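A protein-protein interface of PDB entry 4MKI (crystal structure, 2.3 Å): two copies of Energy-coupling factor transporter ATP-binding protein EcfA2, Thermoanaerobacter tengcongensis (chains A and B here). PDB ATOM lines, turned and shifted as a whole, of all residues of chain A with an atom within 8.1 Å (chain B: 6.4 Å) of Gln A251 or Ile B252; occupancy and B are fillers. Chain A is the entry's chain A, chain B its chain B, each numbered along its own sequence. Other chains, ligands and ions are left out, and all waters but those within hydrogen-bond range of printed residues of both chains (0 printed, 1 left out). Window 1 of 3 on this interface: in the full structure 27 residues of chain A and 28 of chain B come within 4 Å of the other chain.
The backbone NH of Ile B252 sits close to the side-chain amide nitrogen of Gln A251. The side-chain amino group (NZ) of Lys B277 lies within salt-bridge range of the side-chain carboxylate (OE1) of Glu A258, at 3.4 Å.
Of the 19 printed residues of chain A, 7 touch a printed residue of chain B. Among the printed residues, 15 pairs touch across the chains. Among the printed residues, Asp or Glu carboxylates within 4 Å of a Lys or Arg side-chain nitrogen of the other chain: Glu A258 with Lys B277 (3.4 Å).
CG of Glu A209 touches NE2 of Gln B251, 3.5 Å away. Glu B209 touches Gln A251. OE1 of Gln A251 touches NH2 of Arg B213 (3.5 Å). Gln B251 touches Gln A251. Gln A251 touches Ile B273. Ile B252 touches Leu A255 (CD1 to CG, 3.99 Å). O of Ile B273 touches CD2 of Leu A255, 3.8 Å away. CD2 of Leu A255 touches N of Lys B277, at 3.9 Å. Ile A273 touches Gln B251 (CG2 to OE1, 3.5 Å). CD1 of Ile A273 touches CA of Leu B255 (3.9 Å).
OE2 of Glu B209 is in hydrogen-bond range of N of Gln B251 (3.1 Å). OE2 of Glu B274 is in salt-bridge range of NZ of Lys B277 (3.2 Å). The side-chain carboxylate (OE2) of Glu A209 lies within hydrogen-bond range of the backbone NH (N) of Gln A251 (3.1 Å).
Of the printed residues of chain B, Gln A251 touches Glu B209, Arg B213, Gln B251, Ile B252 and Ile B273. Of the printed residues of chain B, Ile A273 touches Gln B251 (3.5 Å) and Leu B255 (3.9 Å). Of the printed residues of chain A, Glu B209 touches Gln A251 (3.6 Å). Of the printed residues of chain A, Ile B252 touches Gln A251 and Leu A255. Leu B271 touches none of the printed residues of chain A. The nearest printed residue of chain B that does not touch Gln A251 is Pro B250 (4.4 Å). The nearest printed residue of chain A that does not touch Ile B252 is Ile A252 (4.6 Å). The nearest printed residue of chain A that does not touch Ile B273 is Ile A252 (5.1 Å).
Glu A209 touches Gln B251, and with the chains exchanged Gln A251 touches Glu B209. Gln B251 touches its own counterpart, Gln A251. Gln A251 touches Ile B252, and with the chains exchanged Ile A252 touches Gln B251. Gln A251 touches Ile B273, and with the chains exchanged Ile A273 touches Gln B251. 14 positions are printed for both chains. Of the 15 pairs that touch across the chains among the printed residues, 11 have their exchanged pair printed and touching as well.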
ATOM      1  N   MET A 208       0.049   0.474 -23.036  1.00  0.00           N
ATOM      2  CA  MET A 208      -0.701   0.592 -24.245  1.00  0.00           C
ATOM      3  C   MET A 208      -0.679   2.033 -24.753  1.00  0.00           C
ATOM      4  O   MET A 208      -0.564   2.256 -25.932  1.00  0.00           O
ATOM      5  CB  MET A 208      -2.135   0.097 -24.001  1.00  0.00           C
ATOM      6  CG  MET A 208      -2.267  -1.362 -23.594  1.00  0.00           C
ATOM      7  SD  MET A 208      -1.634  -2.575 -24.754  1.00  0.00           S
ATOM      8  CE  MET A 208       0.040  -2.856 -24.185  1.00  0.00           C
ATOM      9  N   GLU A 209      -0.728   2.985 -23.825  1.00  0.00           N
ATOM     10  CA  GLU A 209      -0.688   4.405 -24.105  1.00  0.00           C
ATOM     11  C   GLU A 209       0.575   4.806 -24.788  1.00  0.00           C
ATOM     12  O   GLU A 209       0.503   5.522 -25.767  1.00  0.00           O
ATOM     13  CB  GLU A 209      -0.812   5.248 -22.805  1.00  0.00           C
ATOM     14  CG  GLU A 209      -2.223   5.325 -22.205  1.00  0.00           C
ATOM     15  CD  GLU A 209      -2.608   4.108 -21.345  1.00  0.00           C
ATOM     16  OE1 GLU A 209      -1.723   3.265 -21.020  1.00  0.00           O
ATOM     17  OE2 GLU A 209      -3.808   4.019 -20.959  1.00  0.00           O
ATOM     18  N   SER A 248      -5.306  -4.399 -23.467  1.00  0.00           N
ATOM     19  CA  SER A 248      -6.116  -3.272 -23.129  1.00  0.00           C
ATOM     20  C   SER A 248      -5.932  -2.224 -24.224  1.00  0.00           C
ATOM     21  O   SER A 248      -5.055  -2.373 -25.084  1.00  0.00           O
ATOM     22  CB  SER A 248      -5.614  -2.699 -21.825  1.00  0.00           C
ATOM     23  OG  SER A 248      -6.469  -1.674 -21.439  1.00  0.00           O
ATOM     24  N   VAL A 249      -6.749  -1.171 -24.189  1.00  0.00           N
ATOM     25  CA  VAL A 249      -6.559  -0.014 -25.069  1.00  0.00           C
ATOM     26  C   VAL A 249      -6.160   1.177 -24.227  1.00  0.00           C
ATOM     27  O   VAL A 249      -6.315   1.142 -23.046  1.00  0.00           O
ATOM     28  CB  VAL A 249      -7.810   0.290 -25.909  1.00  0.00           C
ATOM     29  CG1 VAL A 249      -8.205  -0.936 -26.714  1.00  0.00           C
ATOM     30  CG2 VAL A 249      -8.997   0.761 -25.073  1.00  0.00           C
ATOM     31  N   PRO A 250      -5.606   2.228 -24.841  1.00  0.00           N
ATOM     32  CA  PRO A 250      -5.335   3.418 -24.069  1.00  0.00           C
ATOM     33  C   PRO A 250      -6.605   3.998 -23.462  1.00  0.00           C
ATOM     34  O   PRO A 250      -7.662   3.911 -24.080  1.00  0.00           O
ATOM     35  CB  PRO A 250      -4.796   4.391 -25.117  1.00  0.00           C
ATOM     36  CG  PRO A 250      -4.224   3.510 -26.207  1.00  0.00           C
ATOM     37  CD  PRO A 250      -5.102   2.317 -26.234  1.00  0.00           C
ATOM     38  N   GLN A 251      -6.502   4.627 -22.288  1.00  0.00           N
ATOM     39  CA  GLN A 251      -7.626   5.317 -21.656  1.00  0.00           C
ATOM     40  C   GLN A 251      -8.447   6.173 -22.636  1.00  0.00           C
ATOM     41  O   GLN A 251      -9.695   6.122 -22.667  1.00  0.00           O
ATOM     42  CB  GLN A 251      -7.143   6.245 -20.526  1.00  0.00           C
ATOM     43  CG  GLN A 251      -7.255   5.757 -19.087  1.00  0.00           C
ATOM     44  CD  GLN A 251      -7.414   6.938 -18.024  1.00  0.00           C
ATOM     45  OE1 GLN A 251      -8.227   6.820 -17.089  1.00  0.00           O
ATOM     46  NE2 GLN A 251      -6.634   8.045 -18.161  1.00  0.00           N
ATOM     47  N   ILE A 252      -7.747   7.014 -23.379  1.00  0.00           N
ATOM     48  CA  ILE A 252      -8.399   7.958 -24.260  1.00  0.00           C
ATOM     49  C   ILE A 252      -9.159   7.241 -25.372  1.00  0.00           C
ATOM     50  O   ILE A 252     -10.257   7.659 -25.778  1.00  0.00           O
ATOM     51  CB  ILE A 252      -7.410   8.976 -24.810  1.00  0.00           C
ATOM     52  CG1 ILE A 252      -8.143  10.112 -25.477  1.00  0.00           C
ATOM     53  CG2 ILE A 252      -6.490   8.364 -25.833  1.00  0.00           C
ATOM     54  CD1 ILE A 252      -8.821  11.008 -24.480  1.00  0.00           C
ATOM     55  N   THR A 253      -8.638   6.109 -25.811  1.00  0.00           N
ATOM     56  CA  THR A 253      -9.368   5.286 -26.764  1.00  0.00           C
ATOM     57  C   THR A 253     -10.643   4.706 -26.150  1.00  0.00           C
ATOM     58  O   THR A 253     -11.662   4.645 -26.828  1.00  0.00           O
ATOM     59  CB  THR A 253      -8.489   4.138 -27.299  1.00  0.00           C
ATOM     60  OG1 THR A 253      -7.233   4.663 -27.729  1.00  0.00           O
ATOM     61  CG2 THR A 253      -9.146   3.465 -28.484  1.00  0.00           C
ATOM     62  N   SER A 254     -10.587   4.227 -24.901  1.00  0.00           N
ATOM     63  CA  SER A 254     -11.786   3.714 -24.245  1.00  0.00           C
ATOM     64  C   SER A 254     -12.867   4.789 -24.160  1.00  0.00           C
ATOM     65  O   SER A 254     -14.043   4.530 -24.403  1.00  0.00           O
ATOM     66  CB  SER A 254     -11.507   3.292 -22.814  1.00  0.00           C
ATOM     67  OG  SER A 254     -10.895   2.038 -22.750  1.00  0.00           O
ATOM     68  N   LEU A 255     -12.467   5.996 -23.796  1.00  0.00           N
ATOM     69  CA  LEU A 255     -13.425   7.106 -23.744  1.00  0.00           C
ATOM     70  C   LEU A 255     -14.101   7.322 -25.118  1.00  0.00           C
ATOM     71  O   LEU A 255     -15.295   7.382 -25.200  1.00  0.00           O
ATOM     72  CB  LEU A 255     -12.699   8.373 -23.262  1.00  0.00           C
ATOM     73  CG  LEU A 255     -13.455   9.653 -22.915  1.00  0.00           C
ATOM     74  CD1 LEU A 255     -13.412  10.615 -24.072  1.00  0.00           C
ATOM     75  CD2 LEU A 255     -14.893   9.401 -22.486  1.00  0.00           C
ATOM     76  N   ALA A 256     -13.315   7.420 -26.190  1.00  0.00           N
ATOM     77  CA  ALA A 256     -13.850   7.643 -27.548  1.00  0.00           C
ATOM     78  C   ALA A 256     -14.852   6.547 -27.907  1.00  0.00           C
ATOM     79  O   ALA A 256     -15.897   6.801 -28.459  1.00  0.00           O
ATOM     80  CB  ALA A 256     -12.714   7.662 -28.557  1.00  0.00           C
ATOM     81  N   ARG A 257     -14.517   5.333 -27.518  1.00  0.00           N
ATOM     82  CA  ARG A 257     -15.347   4.175 -27.653  1.00  0.00           C
ATOM     83  C   ARG A 257     -16.660   4.340 -26.903  1.00  0.00           C
ATOM     84  O   ARG A 257     -17.737   4.026 -27.422  1.00  0.00           O
ATOM     85  CB  ARG A 257     -14.590   3.034 -26.998  1.00  0.00           C
ATOM     86  CG  ARG A 257     -15.083   1.643 -27.304  1.00  0.00           C
ATOM     87  CD  ARG A 257     -14.302   1.112 -28.467  1.00  0.00           C
ATOM     88  NE  ARG A 257     -14.586  -0.297 -28.640  1.00  0.00           N
ATOM     89  CZ  ARG A 257     -14.366  -0.967 -29.760  1.00  0.00           C
ATOM     90  NH1 ARG A 257     -13.837  -0.360 -30.827  1.00  0.00           N
ATOM     91  NH2 ARG A 257     -14.656  -2.270 -29.803  1.00  0.00           N
ATOM     92  N   GLU A 258     -16.567   4.782 -25.655  1.00  0.00           N
ATOM     93  CA  GLU A 258     -17.746   4.939 -24.811  1.00  0.00           C
ATOM     94  C   GLU A 258     -18.663   6.067 -25.275  1.00  0.00           C
ATOM     95  O   GLU A 258     -19.866   5.982 -25.105  1.00  0.00           O
ATOM     96  CB  GLU A 258     -17.344   5.149 -23.355  1.00  0.00           C
ATOM     97  CG  GLU A 258     -16.884   3.874 -22.688  1.00  0.00           C
ATOM     98  CD  GLU A 258     -18.051   3.013 -22.265  1.00  0.00           C
ATOM     99  OE1 GLU A 258     -18.770   3.401 -21.311  1.00  0.00           O
ATOM    100  OE2 GLU A 258     -18.250   1.955 -22.897  1.00  0.00           O
ATOM    101  N   LEU A 259     -18.083   7.119 -25.853  1.00  0.00           N
ATOM    102  CA  LEU A 259     -18.854   8.225 -26.407  1.00  0.00           C
ATOM    103  C   LEU A 259     -19.531   7.794 -27.700  1.00  0.00           C
ATOM    104  O   LEU A 259     -20.678   8.151 -27.939  1.00  0.00           O
ATOM    105  CB  LEU A 259     -17.962   9.429 -26.699  1.00  0.00           C
ATOM    106  CG  LEU A 259     -17.395  10.168 -25.480  1.00  0.00           C
ATOM    107  CD1 LEU A 259     -16.408  11.211 -25.911  1.00  0.00           C
ATOM    108  CD2 LEU A 259     -18.507  10.826 -24.694  1.00  0.00           C
ATOM    109  N   VAL A 270      -9.258   6.787 -31.818  1.00  0.00           N
ATOM    110  CA  VAL A 270      -8.494   7.912 -31.333  1.00  0.00           C
ATOM    111  C   VAL A 270      -7.358   7.372 -30.467  1.00  0.00           C
ATOM    112  O   VAL A 270      -7.595   6.550 -29.579  1.00  0.00           O
ATOM    113  CB  VAL A 270      -9.429   8.827 -30.492  1.00  0.00           C
ATOM    114  CG1 VAL A 270      -8.654   9.804 -29.633  1.00  0.00           C
ATOM    115  CG2 VAL A 270     -10.381   9.559 -31.413  1.00  0.00           C
ATOM    116  N   LEU A 271      -6.150   7.859 -30.684  1.00  0.00           N
ATOM    117  CA  LEU A 271      -4.995   7.329 -29.958  1.00  0.00           C
ATOM    118  C   LEU A 271      -4.398   8.245 -28.917  1.00  0.00           C
ATOM    119  O   LEU A 271      -3.749   7.759 -28.020  1.00  0.00           O
ATOM    120  CB  LEU A 271      -3.879   6.990 -30.928  1.00  0.00           C
ATOM    121  CG  LEU A 271      -4.204   6.022 -32.044  1.00  0.00           C
ATOM    122  CD1 LEU A 271      -2.998   5.898 -32.935  1.00  0.00           C
ATOM    123  CD2 LEU A 271      -4.647   4.683 -31.481  1.00  0.00           C
ATOM    124  N   ILE A 273      -4.558  12.199 -26.511  1.00  0.00           N
ATOM    125  CA  ILE A 273      -5.368  13.293 -25.994  1.00  0.00           C
ATOM    126  C   ILE A 273      -5.536  14.382 -27.076  1.00  0.00           C
ATOM    127  O   ILE A 273      -6.642  14.855 -27.310  1.00  0.00           O
ATOM    128  CB  ILE A 273      -4.880  13.913 -24.603  1.00  0.00           C
ATOM    129  CG1 ILE A 273      -4.310  15.340 -24.720  1.00  0.00           C
ATOM    130  CG2 ILE A 273      -3.961  13.007 -23.759  1.00  0.00           C
ATOM    131  CD1 ILE A 273      -5.373  16.420 -24.704  1.00  0.00           C
ATOM    132  N   ALA A 276      -8.155  13.371 -29.575  1.00  0.00           N
ATOM    133  CA  ALA A 276      -9.468  13.343 -28.974  1.00  0.00           C
ATOM    134  C   ALA A 276     -10.034  14.740 -28.795  1.00  0.00           C
ATOM    135  O   ALA A 276     -11.226  14.975 -29.038  1.00  0.00           O
ATOM    136  CB  ALA A 276      -9.410  12.655 -27.630  1.00  0.00           C
ATOM    137  N   ILE A 280     -13.434  16.145 -30.608  1.00  0.00           N
ATOM    138  CA  ILE A 280     -14.536  16.515 -29.741  1.00  0.00           C
ATOM    139  C   ILE A 280     -14.900  17.981 -29.984  1.00  0.00           C
ATOM    140  O   ILE A 280     -16.067  18.323 -30.152  1.00  0.00           O
ATOM    141  CB  ILE A 280     -14.175  16.279 -28.284  1.00  0.00           C
ATOM    142  CG1 ILE A 280     -14.048  14.781 -28.045  1.00  0.00           C
ATOM    143  CG2 ILE A 280     -15.255  16.859 -27.382  1.00  0.00           C
ATOM    144  CD1 ILE A 280     -13.480  14.428 -26.690  1.00  0.00           C
ATOM    145  N   GLU B 209      -2.568   7.345 -13.291  1.00  0.00           N
ATOM    146  CA  GLU B 209      -3.915   6.841 -13.635  1.00  0.00           C
ATOM    147  C   GLU B 209      -4.435   5.868 -12.613  1.00  0.00           C
ATOM    148  O   GLU B 209      -5.561   6.006 -12.160  1.00  0.00           O
ATOM    149  CB  GLU B 209      -3.918   6.133 -14.987  1.00  0.00           C
ATOM    150  CG  GLU B 209      -3.823   7.048 -16.211  1.00  0.00           C
ATOM    151  CD  GLU B 209      -2.400   7.464 -16.588  1.00  0.00           C
ATOM    152  OE1 GLU B 209      -1.402   6.958 -15.994  1.00  0.00           O
ATOM    153  OE2 GLU B 209      -2.273   8.302 -17.506  1.00  0.00           O
ATOM    154  N   ARG B 213      -7.610   6.571  -9.560  1.00  0.00           N
ATOM    155  CA  ARG B 213      -8.868   5.813  -9.491  1.00  0.00           C
ATOM    156  C   ARG B 213      -9.096   5.241  -8.093  1.00  0.00           C
ATOM    157  O   ARG B 213     -10.192   5.175  -7.651  1.00  0.00           O
ATOM    158  CB  ARG B 213      -8.889   4.627 -10.488  1.00  0.00           C
ATOM    159  CG  ARG B 213      -8.922   5.042 -11.964  1.00  0.00           C
ATOM    160  CD  ARG B 213      -8.867   3.864 -12.995  1.00  0.00           C
ATOM    161  NE  ARG B 213      -9.343   4.375 -14.289  1.00  0.00           N
ATOM    162  CZ  ARG B 213     -10.638   4.426 -14.694  1.00  0.00           C
ATOM    163  NH1 ARG B 213     -11.623   3.897 -13.953  1.00  0.00           N
ATOM    164  NH2 ARG B 213     -10.965   5.010 -15.860  1.00  0.00           N
ATOM    165  N   VAL B 249      -0.211  14.233 -14.558  1.00  0.00           N
ATOM    166  CA  VAL B 249      -1.610  13.934 -14.261  1.00  0.00           C
ATOM    167  C   VAL B 249      -2.089  12.807 -15.174  1.00  0.00           C
ATOM    168  O   VAL B 249      -1.430  12.479 -16.128  1.00  0.00           O
ATOM    169  CB  VAL B 249      -2.515  15.158 -14.443  1.00  0.00           C
ATOM    170  CG1 VAL B 249      -1.989  16.277 -13.601  1.00  0.00           C
ATOM    171  CG2 VAL B 249      -2.637  15.610 -15.898  1.00  0.00           C
ATOM    172  N   PRO B 250      -3.199  12.169 -14.849  1.00  0.00           N
ATOM    173  CA  PRO B 250      -3.691  11.123 -15.726  1.00  0.00           C
ATOM    174  C   PRO B 250      -4.051  11.662 -17.094  1.00  0.00           C
ATOM    175  O   PRO B 250      -4.486  12.798 -17.168  1.00  0.00           O
ATOM    176  CB  PRO B 250      -5.002  10.663 -15.030  1.00  0.00           C
ATOM    177  CG  PRO B 250      -4.779  10.938 -13.576  1.00  0.00           C
ATOM    178  CD  PRO B 250      -3.919  12.205 -13.559  1.00  0.00           C
ATOM    179  N   GLN B 251      -3.905  10.855 -18.153  1.00  0.00           N
ATOM    180  CA  GLN B 251      -4.260  11.284 -19.503  1.00  0.00           C
ATOM    181  C   GLN B 251      -5.641  11.943 -19.532  1.00  0.00           C
ATOM    182  O   GLN B 251      -5.839  12.987 -20.150  1.00  0.00           O
ATOM    183  CB  GLN B 251      -4.212  10.123 -20.517  1.00  0.00           C
ATOM    184  CG  GLN B 251      -2.905   9.954 -21.353  1.00  0.00           C
ATOM    185  CD  GLN B 251      -3.130   9.332 -22.789  1.00  0.00           C
ATOM    186  OE1 GLN B 251      -2.531   9.810 -23.757  1.00  0.00           O
ATOM    187  NE2 GLN B 251      -4.023   8.291 -22.930  1.00  0.00           N
ATOM    188  N   ILE B 252      -6.608  11.302 -18.917  1.00  0.00           N
ATOM    189  CA  ILE B 252      -7.984  11.764 -19.008  1.00  0.00           C
ATOM    190  C   ILE B 252      -8.133  13.135 -18.331  1.00  0.00           C
ATOM    191  O   ILE B 252      -8.943  13.951 -18.792  1.00  0.00           O
ATOM    192  CB  ILE B 252      -9.015  10.739 -18.444  1.00  0.00           C
ATOM    193  CG1 ILE B 252     -10.442  11.115 -18.796  1.00  0.00           C
ATOM    194  CG2 ILE B 252      -8.959  10.642 -16.939  1.00  0.00           C
ATOM    195  CD1 ILE B 252     -10.750  10.900 -20.254  1.00  0.00           C
ATOM    196  N   THR B 253      -7.369  13.366 -17.268  1.00  0.00           N
ATOM    197  CA  THR B 253      -7.362  14.642 -16.629  1.00  0.00           C
ATOM    198  C   THR B 253      -6.804  15.703 -17.545  1.00  0.00           C
ATOM    199  O   THR B 253      -7.349  16.773 -17.592  1.00  0.00           O
ATOM    200  CB  THR B 253      -6.575  14.628 -15.324  1.00  0.00           C
ATOM    201  OG1 THR B 253      -7.047  13.541 -14.529  1.00  0.00           O
ATOM    202  CG2 THR B 253      -6.764  15.918 -14.521  1.00  0.00           C
ATOM    203  N   SER B 254      -5.707  15.415 -18.254  1.00  0.00           N
ATOM    204  CA  SER B 254      -5.142  16.359 -19.217  1.00  0.00           C
ATOM    205  C   SER B 254      -6.150  16.717 -20.248  1.00  0.00           C
ATOM    206  O   SER B 254      -6.256  17.871 -20.648  1.00  0.00           O
ATOM    207  CB  SER B 254      -3.945  15.774 -19.969  1.00  0.00           C
ATOM    208  OG  SER B 254      -2.799  15.752 -19.177  1.00  0.00           O
ATOM    209  N   LEU B 255      -6.880  15.723 -20.733  1.00  0.00           N
ATOM    210  CA  LEU B 255      -7.870  15.978 -21.760  1.00  0.00           C
ATOM    211  C   LEU B 255      -8.940  16.915 -21.208  1.00  0.00           C
ATOM    212  O   LEU B 255      -9.225  17.917 -21.825  1.00  0.00           O
ATOM    213  CB  LEU B 255      -8.459  14.668 -22.256  1.00  0.00           C
ATOM    214  CG  LEU B 255      -9.417  14.584 -23.458  1.00  0.00           C
ATOM    215  CD1 LEU B 255     -10.841  14.515 -23.002  1.00  0.00           C
ATOM    216  CD2 LEU B 255      -9.215  15.699 -24.461  1.00  0.00           C
ATOM    217  N   ALA B 256      -9.486  16.606 -20.041  1.00  0.00           N
ATOM    218  CA  ALA B 256     -10.510  17.444 -19.463  1.00  0.00           C
ATOM    219  C   ALA B 256     -10.028  18.882 -19.355  1.00  0.00           C
ATOM    220  O   ALA B 256     -10.801  19.803 -19.599  1.00  0.00           O
ATOM    221  CB  ALA B 256     -10.893  16.969 -18.088  1.00  0.00           C
ATOM    222  N   ARG B 257      -8.779  19.040 -18.930  1.00  0.00           N
ATOM    223  CA  ARG B 257      -8.160  20.336 -18.758  1.00  0.00           C
ATOM    224  C   ARG B 257      -8.164  21.062 -20.081  1.00  0.00           C
ATOM    225  O   ARG B 257      -8.502  22.234 -20.138  1.00  0.00           O
ATOM    226  CB  ARG B 257      -6.690  20.214 -18.331  1.00  0.00           C
ATOM    227  CG  ARG B 257      -6.413  19.938 -16.885  1.00  0.00           C
ATOM    228  CD  ARG B 257      -4.914  19.781 -16.622  1.00  0.00           C
ATOM    229  NE  ARG B 257      -4.274  21.097 -16.594  1.00  0.00           N
ATOM    230  CZ  ARG B 257      -4.369  21.961 -15.577  1.00  0.00           C
ATOM    231  NH1 ARG B 257      -5.053  21.640 -14.464  1.00  0.00           N
ATOM    232  NH2 ARG B 257      -3.767  23.153 -15.661  1.00  0.00           N
ATOM    233  N   VAL B 270     -11.382  15.860 -13.512  1.00  0.00           N
ATOM    234  CA  VAL B 270     -11.960  14.563 -13.894  1.00  0.00           C
ATOM    235  C   VAL B 270     -10.850  13.557 -13.777  1.00  0.00           C
ATOM    236  O   VAL B 270      -9.714  13.830 -14.196  1.00  0.00           O
ATOM    237  CB  VAL B 270     -12.411  14.642 -15.364  1.00  0.00           C
ATOM    238  CG1 VAL B 270     -12.612  13.278 -16.001  1.00  0.00           C
ATOM    239  CG2 VAL B 270     -13.683  15.466 -15.454  1.00  0.00           C
ATOM    240  N   LEU B 271     -11.146  12.433 -13.154  1.00  0.00           N
ATOM    241  CA  LEU B 271     -10.124  11.431 -12.819  1.00  0.00           C
ATOM    242  C   LEU B 271     -10.279  10.111 -13.588  1.00  0.00           C
ATOM    243  O   LEU B 271      -9.306   9.341 -13.643  1.00  0.00           O
ATOM    244  CB  LEU B 271     -10.161  11.081 -11.315  1.00  0.00           C
ATOM    245  CG  LEU B 271     -10.001  12.192 -10.287  1.00  0.00           C
ATOM    246  CD1 LEU B 271     -10.193  11.622  -8.893  1.00  0.00           C
ATOM    247  CD2 LEU B 271      -8.651  12.876 -10.431  1.00  0.00           C
ATOM    248  N   THR B 272     -11.480   9.850 -14.114  1.00  0.00           N
ATOM    249  CA  THR B 272     -11.810   8.604 -14.806  1.00  0.00           C
ATOM    250  C   THR B 272     -12.530   8.795 -16.158  1.00  0.00           C
ATOM    251  O   THR B 272     -13.252   9.769 -16.371  1.00  0.00           O
ATOM    252  CB  THR B 272     -12.775   7.757 -13.980  1.00  0.00           C
ATOM    253  OG1 THR B 272     -14.050   8.410 -13.973  1.00  0.00           O
ATOM    254  CG2 THR B 272     -12.292   7.558 -12.533  1.00  0.00           C
ATOM    255  N   ILE B 273     -12.367   7.841 -17.072  1.00  0.00           N
ATOM    256  CA  ILE B 273     -13.111   7.923 -18.345  1.00  0.00           C
ATOM    257  C   ILE B 273     -14.621   7.993 -18.111  1.00  0.00           C
ATOM    258  O   ILE B 273     -15.316   8.781 -18.732  1.00  0.00           O
ATOM    259  CB  ILE B 273     -12.729   6.842 -19.413  1.00  0.00           C
ATOM    260  CG1 ILE B 273     -13.075   5.474 -18.950  1.00  0.00           C
ATOM    261  CG2 ILE B 273     -11.258   6.907 -19.724  1.00  0.00           C
ATOM    262  CD1 ILE B 273     -12.407   4.379 -19.746  1.00  0.00           C
ATOM    263  N   GLU B 274     -15.101   7.214 -17.169  1.00  0.00           N
ATOM    264  CA  GLU B 274     -16.503   7.262 -16.825  1.00  0.00           C
ATOM    265  C   GLU B 274     -16.987   8.681 -16.472  1.00  0.00           C
ATOM    266  O   GLU B 274     -18.003   9.149 -16.983  1.00  0.00           O
ATOM    267  CB  GLU B 274     -16.750   6.286 -15.689  1.00  0.00           C
ATOM    268  CG  GLU B 274     -17.819   5.255 -15.989  1.00  0.00           C
ATOM    269  CD  GLU B 274     -19.241   5.805 -15.865  1.00  0.00           C
ATOM    270  OE1 GLU B 274     -19.436   6.982 -15.463  1.00  0.00           O
ATOM    271  OE2 GLU B 274     -20.182   5.041 -16.176  1.00  0.00           O
ATOM    272  N   ALA B 276     -15.603  11.528 -17.308  1.00  0.00           N
ATOM    273  CA  ALA B 276     -15.441  12.388 -18.441  1.00  0.00           C
ATOM    274  C   ALA B 276     -16.595  12.151 -19.435  1.00  0.00           C
ATOM    275  O   ALA B 276     -17.105  13.074 -20.063  1.00  0.00           O
ATOM    276  CB  ALA B 276     -14.110  12.110 -19.088  1.00  0.00           C
ATOM    277  N   LYS B 277     -16.975  10.891 -19.602  1.00  0.00           N
ATOM    278  CA  LYS B 277     -18.100  10.514 -20.476  1.00  0.00           C
ATOM    279  C   LYS B 277     -19.396  11.204 -20.020  1.00  0.00           C
ATOM    280  O   LYS B 277     -20.064  11.857 -20.813  1.00  0.00           O
ATOM    281  CB  LYS B 277     -18.255   8.993 -20.466  1.00  0.00           C
ATOM    282  CG  LYS B 277     -19.380   8.454 -21.361  1.00  0.00           C
ATOM    283  CD  LYS B 277     -20.333   7.560 -20.564  1.00  0.00           C
ATOM    284  CE  LYS B 277     -19.651   6.305 -20.040  1.00  0.00           C
ATOM    285  NZ  LYS B 277     -20.649   5.468 -19.315  1.00  0.00           N
